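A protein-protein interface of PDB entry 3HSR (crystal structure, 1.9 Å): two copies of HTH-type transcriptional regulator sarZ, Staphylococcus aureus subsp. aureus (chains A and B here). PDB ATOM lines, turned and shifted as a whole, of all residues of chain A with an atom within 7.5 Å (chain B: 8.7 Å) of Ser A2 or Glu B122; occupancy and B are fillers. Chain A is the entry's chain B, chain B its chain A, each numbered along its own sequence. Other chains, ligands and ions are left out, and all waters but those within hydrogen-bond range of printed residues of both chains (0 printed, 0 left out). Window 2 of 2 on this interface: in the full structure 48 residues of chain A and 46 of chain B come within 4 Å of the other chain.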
ATOM      1  N   GLY A   1      35.409  -7.748   3.403  1.00  0.00           N
ATOM      2  CA  GLY A   1      35.777  -6.308   3.384  1.00  0.00           C
ATOM      3  C   GLY A   1      34.685  -5.446   3.965  1.00  0.00           C
ATOM      4  O   GLY A   1      33.764  -5.974   4.585  1.00  0.00           O
ATOM      5  N   SER A   2      34.773  -4.133   3.775  1.00  0.00           N
ATOM      6  CA  SER A   2      33.918  -3.208   4.520  1.00  0.00           C
ATOM      7  C   SER A   2      32.419  -3.392   4.246  1.00  0.00           C
ATOM      8  O   SER A   2      31.586  -3.211   5.146  1.00  0.00           O
ATOM      9  CB  SER A   2      34.299  -1.757   4.221  1.00  0.00           C
ATOM     10  OG  SER A   2      34.180  -1.526   2.829  1.00  0.00           O
ATOM     11  N   HIS A   3      32.073  -3.738   3.010  1.00  0.00           N
ATOM     12  CA  HIS A   3      30.674  -4.007   2.716  1.00  0.00           C
ATOM     13  C   HIS A   3      30.122  -5.113   3.612  1.00  0.00           C
ATOM     14  O   HIS A   3      28.950  -5.091   3.956  1.00  0.00           O
ATOM     15  CB  HIS A   3      30.475  -4.299   1.221  1.00  0.00           C
ATOM     16  CG  HIS A   3      30.696  -3.105   0.345  1.00  0.00           C
ATOM     17  ND1 HIS A   3      31.541  -2.071   0.695  1.00  0.00           N
ATOM     18  CD2 HIS A   3      30.214  -2.797  -0.885  1.00  0.00           C
ATOM     19  CE1 HIS A   3      31.561  -1.174  -0.277  1.00  0.00           C
ATOM     20  NE2 HIS A   3      30.778  -1.600  -1.254  1.00  0.00           N
ATOM     21  N   MET A   4      30.939  -6.082   4.014  1.00  0.00           N
ATOM     22  CA  MET A   4      30.459  -7.158   4.869  1.00  0.00           C
ATOM     23  C   MET A   4      30.447  -6.745   6.354  1.00  0.00           C
ATOM     24  O   MET A   4      29.462  -6.959   7.068  1.00  0.00           O
ATOM     25  CB  MET A   4      31.271  -8.446   4.636  1.00  0.00           C
ATOM     26  CG  MET A   4      30.893  -9.641   5.525  1.00  0.00           C
ATOM     27  SD  MET A   4      29.182 -10.161   5.292  1.00  0.00           S
ATOM     28  CE  MET A   4      29.345 -11.194   3.822  1.00  0.00           C
ATOM     29  N   TYR A   5      31.544  -6.167   6.825  1.00  0.00           N
ATOM     30  CA  TYR A   5      31.618  -5.905   8.257  1.00  0.00           C
ATOM     31  C   TYR A   5      30.766  -4.739   8.678  1.00  0.00           C
ATOM     32  O   TYR A   5      30.138  -4.795   9.720  1.00  0.00           O
ATOM     33  CB  TYR A   5      33.062  -5.858   8.807  1.00  0.00           C
ATOM     34  CG  TYR A   5      33.974  -4.783   8.297  1.00  0.00           C
ATOM     35  CD1 TYR A   5      35.013  -5.093   7.410  1.00  0.00           C
ATOM     36  CD2 TYR A   5      33.843  -3.452   8.739  1.00  0.00           C
ATOM     37  CE1 TYR A   5      35.854  -4.091   6.924  1.00  0.00           C
ATOM     38  CE2 TYR A   5      34.675  -2.472   8.268  1.00  0.00           C
ATOM     39  CZ  TYR A   5      35.684  -2.807   7.357  1.00  0.00           C
ATOM     40  OH  TYR A   5      36.527  -1.821   6.911  1.00  0.00           O
ATOM     41  N   LEU A   6      30.687  -3.707   7.868  1.00  0.00           N
ATOM     42  CA  LEU A   6      29.816  -2.612   8.188  1.00  0.00           C
ATOM     43  C   LEU A   6      28.342  -3.008   8.110  1.00  0.00           C
ATOM     44  O   LEU A   6      27.530  -2.541   8.934  1.00  0.00           O
ATOM     45  CB  LEU A   6      30.092  -1.403   7.289  1.00  0.00           C
ATOM     46  CG  LEU A   6      31.514  -0.840   7.359  1.00  0.00           C
ATOM     47  CD1 LEU A   6      31.719   0.258   6.328  1.00  0.00           C
ATOM     48  CD2 LEU A   6      31.873  -0.356   8.780  1.00  0.00           C
ATOM     49  N   SER A   7      27.966  -3.855   7.134  1.00  0.00           N
ATOM     50  CA  SER A   7      26.545  -4.158   6.950  1.00  0.00           C
ATOM     51  C   SER A   7      26.039  -5.043   8.075  1.00  0.00           C
ATOM     52  O   SER A   7      24.893  -4.909   8.506  1.00  0.00           O
ATOM     53  CB  SER A   7      26.273  -4.832   5.599  1.00  0.00           C
ATOM     54  OG  SER A   7      24.879  -5.054   5.452  1.00  0.00           O
ATOM     55  N   LYS A   8      26.889  -5.949   8.528  1.00  0.00           N
ATOM     56  CA  LYS A   8      26.577  -6.815   9.635  1.00  0.00           C
ATOM     57  C   LYS A   8      26.279  -5.991  10.904  1.00  0.00           C
ATOM     58  O   LYS A   8      25.328  -6.319  11.643  1.00  0.00           O
ATOM     59  CB  LYS A   8      27.762  -7.738   9.903  1.00  0.00           C
ATOM     60  CG  LYS A   8      27.864  -8.884   8.962  1.00  0.00           C
ATOM     61  CD  LYS A   8      29.158  -9.607   9.285  1.00  0.00           C
ATOM     62  CE  LYS A   8      29.120 -11.041   8.738  1.00  0.00           C
ATOM     63  NZ  LYS A   8      30.424 -11.766   8.887  1.00  0.00           N
ATOM     64  N   SER B 111      23.006  -9.446   4.048  1.00  0.00           N
ATOM     65  CA  SER B 111      23.165  -8.149   4.696  1.00  0.00           C
ATOM     66  C   SER B 111      23.896  -7.157   3.797  1.00  0.00           C
ATOM     67  O   SER B 111      23.530  -5.982   3.766  1.00  0.00           O
ATOM     68  CB  SER B 111      23.855  -8.260   6.063  1.00  0.00           C
ATOM     69  OG  SER B 111      25.172  -8.759   5.942  1.00  0.00           O
ATOM     70  N   VAL B 112      24.919  -7.623   3.075  1.00  0.00           N
ATOM     71  CA  VAL B 112      25.643  -6.801   2.112  1.00  0.00           C
ATOM     72  C   VAL B 112      24.745  -6.328   0.939  1.00  0.00           C
ATOM     73  O   VAL B 112      24.746  -5.157   0.595  1.00  0.00           O
ATOM     74  CB  VAL B 112      26.802  -7.550   1.494  1.00  0.00           C
ATOM     75  CG1 VAL B 112      27.456  -6.733   0.390  1.00  0.00           C
ATOM     76  CG2 VAL B 112      27.837  -7.925   2.544  1.00  0.00           C
ATOM     77  N   PHE B 115      22.076  -3.482   2.793  1.00  0.00           N
ATOM     78  CA  PHE B 115      22.566  -2.145   3.151  1.00  0.00           C
ATOM     79  C   PHE B 115      23.242  -1.460   1.936  1.00  0.00           C
ATOM     80  O   PHE B 115      23.277  -0.229   1.814  1.00  0.00           O
ATOM     81  CB  PHE B 115      23.399  -2.214   4.440  1.00  0.00           C
ATOM     82  CG  PHE B 115      22.545  -2.511   5.679  1.00  0.00           C
ATOM     83  CD1 PHE B 115      21.816  -1.492   6.293  1.00  0.00           C
ATOM     84  CD2 PHE B 115      22.403  -3.815   6.154  1.00  0.00           C
ATOM     85  CE1 PHE B 115      20.994  -1.771   7.392  1.00  0.00           C
ATOM     86  CE2 PHE B 115      21.580  -4.114   7.258  1.00  0.00           C
ATOM     87  CZ  PHE B 115      20.886  -3.095   7.881  1.00  0.00           C
ATOM     88  N   ASN B 119      22.304   4.190  -0.702  1.00  0.00           N
ATOM     89  CA  ASN B 119      23.460   4.878  -1.218  1.00  0.00           C
ATOM     90  C   ASN B 119      24.130   5.363   0.045  1.00  0.00           C
ATOM     91  O   ASN B 119      23.689   6.356   0.652  1.00  0.00           O
ATOM     92  CB  ASN B 119      23.034   6.071  -2.060  1.00  0.00           C
ATOM     93  CG  ASN B 119      24.188   6.679  -2.806  1.00  0.00           C
ATOM     94  OD1 ASN B 119      25.255   6.061  -2.925  1.00  0.00           O
ATOM     95  ND2 ASN B 119      23.991   7.887  -3.321  1.00  0.00           N
ATOM     96  N   ILE B 120      25.111   4.613   0.525  1.00  0.00           N
ATOM     97  CA  ILE B 120      25.713   4.956   1.782  1.00  0.00           C
ATOM     98  C   ILE B 120      27.224   4.667   1.722  1.00  0.00           C
ATOM     99  O   ILE B 120      27.626   3.586   1.301  1.00  0.00           O
ATOM    100  CB  ILE B 120      24.978   4.206   2.925  1.00  0.00           C
ATOM    101  CG1 ILE B 120      25.586   4.456   4.267  1.00  0.00           C
ATOM    102  CG2 ILE B 120      24.966   2.686   2.710  1.00  0.00           C
ATOM    103  CD1 ILE B 120      24.945   3.530   5.327  1.00  0.00           C
ATOM    104  N   SER B 121      28.058   5.640   2.101  1.00  0.00           N
ATOM    105  CA  SER B 121      29.516   5.406   2.078  1.00  0.00           C
ATOM    106  C   SER B 121      30.030   4.612   3.296  1.00  0.00           C
ATOM    107  O   SER B 121      29.291   4.358   4.259  1.00  0.00           O
ATOM    108  CB  SER B 121      30.280   6.720   1.974  1.00  0.00           C
ATOM    109  OG  SER B 121      30.053   7.538   3.116  1.00  0.00           O
ATOM    110  N   GLU B 122      31.311   4.242   3.266  1.00  0.00           N
ATOM    111  CA  GLU B 122      31.924   3.616   4.444  1.00  0.00           C
ATOM    112  C   GLU B 122      31.896   4.575   5.637  1.00  0.00           C
ATOM    113  O   GLU B 122      31.528   4.180   6.736  1.00  0.00           O
ATOM    114  CB  GLU B 122      33.367   3.157   4.178  1.00  0.00           C
ATOM    115  CG  GLU B 122      33.514   2.000   3.207  1.00  0.00           C
ATOM    116  CD  GLU B 122      34.990   1.595   3.010  1.00  0.00           C
ATOM    117  OE1 GLU B 122      35.894   2.316   3.495  1.00  0.00           O
ATOM    118  OE2 GLU B 122      35.247   0.537   2.396  1.00  0.00           O
ATOM    119  N   ARG B 123      32.259   5.833   5.406  1.00  0.00           N
ATOM    120  CA  ARG B 123      32.225   6.831   6.469  1.00  0.00           C
ATOM    121  C   ARG B 123      30.802   7.087   7.000  1.00  0.00           C
ATOM    122  O   ARG B 123      30.611   7.256   8.200  1.00  0.00           O
ATOM    123  CB  ARG B 123      32.875   8.138   6.003  1.00  0.00           C
ATOM    124  CG  ARG B 123      32.525   9.344   6.873  1.00  0.00           C
ATOM    125  CD  ARG B 123      33.576  10.482   6.778  1.00  0.00           C
ATOM    126  NE  ARG B 123      33.543  11.391   7.943  1.00  0.00           N
ATOM    127  CZ  ARG B 123      33.767  10.990   9.195  1.00  0.00           C
ATOM    128  NH1 ARG B 123      34.035   9.716   9.428  1.00  0.00           N
ATOM    129  NH2 ARG B 123      33.725  11.848  10.199  1.00  0.00           N
ATOM    130  N   GLU B 124      29.815   7.122   6.100  1.00  0.00           N
ATOM    131  CA  GLU B 124      28.417   7.321   6.507  1.00  0.00           C
ATOM    132  C   GLU B 124      27.925   6.114   7.336  1.00  0.00           C
ATOM    133  O   GLU B 124      27.280   6.262   8.392  1.00  0.00           O
ATOM    134  CB  GLU B 124      27.547   7.536   5.244  1.00  0.00           C
ATOM    135  CG  GLU B 124      27.628   8.923   4.697  1.00  0.00           C
ATOM    136  CD  GLU B 124      26.972   9.040   3.332  1.00  0.00           C
ATOM    137  OE1 GLU B 124      26.582   8.013   2.750  1.00  0.00           O
ATOM    138  OE2 GLU B 124      26.828  10.167   2.851  1.00  0.00           O
ATOM    139  N   ALA B 125      28.256   4.912   6.886  1.00  0.00           N
ATOM    140  CA  ALA B 125      27.883   3.744   7.646  1.00  0.00           C
ATOM    141  C   ALA B 125      28.567   3.736   9.036  1.00  0.00           C
ATOM    142  O   ALA B 125      27.968   3.312  10.030  1.00  0.00           O
ATOM    143  CB  ALA B 125      28.254   2.473   6.888  1.00  0.00           C
ATOM    144  N   SER B 126      29.840   4.132   9.074  1.00  0.00           N
ATOM    145  CA  SER B 126      30.627   4.087  10.345  1.00  0.00           C
ATOM    146  C   SER B 126      30.017   5.045  11.343  1.00  0.00           C
ATOM    147  O   SER B 126      29.943   4.745  12.546  1.00  0.00           O
ATOM    148  CB  SER B 126      32.082   4.518  10.091  1.00  0.00           C
ATOM    149  OG  SER B 126      32.734   3.562   9.271  1.00  0.00           O
ATOM    150  N   ASP B 127      29.601   6.215  10.869  1.00  0.00           N
ATOM    151  CA  ASP B 127      28.983   7.209  11.763  1.00  0.00           C
ATOM    152  C   ASP B 127      27.684   6.672  12.335  1.00  0.00           C
ATOM    153  O   ASP B 127      27.394   6.851  13.509  1.00  0.00           O
ATOM    154  CB  ASP B 127      28.672   8.518  11.036  1.00  0.00           C
ATOM    155  CG  ASP B 127      29.898   9.338  10.751  1.00  0.00           C
ATOM    156  OD1 ASP B 127      30.975   8.975  11.247  1.00  0.00           O
ATOM    157  OD2 ASP B 127      29.787  10.362  10.022  1.00  0.00           O
ATOM    158  N   ILE B 128      26.874   6.026  11.492  1.00  0.00           N
ATOM    159  CA  ILE B 128      25.619   5.470  11.964  1.00  0.00           C
ATOM    160  C   ILE B 128      25.871   4.380  12.979  1.00  0.00           C
ATOM    161  O   ILE B 128      25.232   4.364  14.027  1.00  0.00           O
ATOM    162  CB  ILE B 128      24.732   4.883  10.790  1.00  0.00           C
ATOM    163  CG1 ILE B 128      24.159   6.052  10.002  1.00  0.00           C
ATOM    164  CG2 ILE B 128      23.641   4.055  11.403  1.00  0.00           C
ATOM    165  CD1 ILE B 128      23.534   5.701   8.622  1.00  0.00           C
ATOM    166  N   ILE B 129      26.815   3.488  12.672  1.00  0.00           N
ATOM    167  CA  ILE B 129      27.238   2.445  13.594  1.00  0.00           C
ATOM    168  C   ILE B 129      27.698   3.003  14.930  1.00  0.00           C
ATOM    169  O   ILE B 129      27.272   2.509  15.976  1.00  0.00           O
ATOM    170  CB  ILE B 129      28.329   1.561  12.981  1.00  0.00           C
ATOM    171  CG1 ILE B 129      27.732   0.731  11.829  1.00  0.00           C
ATOM    172  CG2 ILE B 129      29.001   0.641  14.044  1.00  0.00           C
ATOM    173  CD1 ILE B 129      28.806   0.172  10.880  1.00  0.00           C
ATOM    174  N   ASN B 130      28.579   3.999  14.913  1.00  0.00           N
ATOM    175  CA  ASN B 130      29.021   4.573  16.196  1.00  0.00           C
ATOM    176  C   ASN B 130      27.827   5.166  16.995  1.00  0.00           C
ATOM    177  O   ASN B 130      27.770   5.011  18.208  1.00  0.00           O
ATOM    178  CB  ASN B 130      30.095   5.620  15.951  1.00  0.00           C
ATOM    179  CG  ASN B 130      31.382   5.005  15.436  1.00  0.00           C
ATOM    180  OD1 ASN B 130      32.119   5.620  14.654  1.00  0.00           O
ATOM    181  ND2 ASN B 130      31.653   3.788  15.861  1.00  0.00           N
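The side-chain hydroxyl (OG) of Ser A2 lies close to the side-chain carboxylate (OE2) of Glu B122 (2.4 Å).
OG of Ser A7 lies close to O of Ser B111 (2.4 Å).
The backbone carbonyl oxygen (O) of Glu B122 lies within hydrogen-bond range of the side-chain hydroxyl (OG) of Ser B126.
ND1 of His A3 lies within hydrogen-bond range of OG of Ser A2 (3.4 Å).
Among the printed residues, pairs that only touch across the chains: His A3 with Val B112, Met A4 with Val B112, Leu A6 with Glu B122, Leu A6 with Ile B129, Ser A7 with Val B112 and Ser A7 with Phe B115.
Ser A2 touches one residue of chain B.
Printed residues of chain B within 4 Å of Met A4: Val B112.
Tyr A5 touches none of the printed residues of chain B.
Lys A8 touches none of the printed residues of chain B.
Printed residues of chain A within 4 Å of Ser B111: Ser A7.
Of the printed residues of chain A, Val B112 touches His A3, Met A4 and Ser A7.
The nearest residue of chain B that does not touch Ser A2 is Val B112 (6.6 Å).
The nearest residue of chain A that does not touch Glu B122 is His A3 (4.8 Å).
Of the 8 printed residues of chain A, 5 touch a printed residue of chain B.
Hydrophobic or aromatic side chains of chain B within 4 Å of the printed part of chain A: Val B112, Phe B115 and Ile B129.
Among the printed residues, 8 pairs touch across the chains.
Among the printed residues, no Asp or Glu carboxylate lies within 4 Å of a Lys or Arg side-chain nitrogen of the other chain.
No position is printed for both chains.
Of the 8 pairs that touch across the chains among the printed residues, none has its exchanged pair printed and touching as well.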
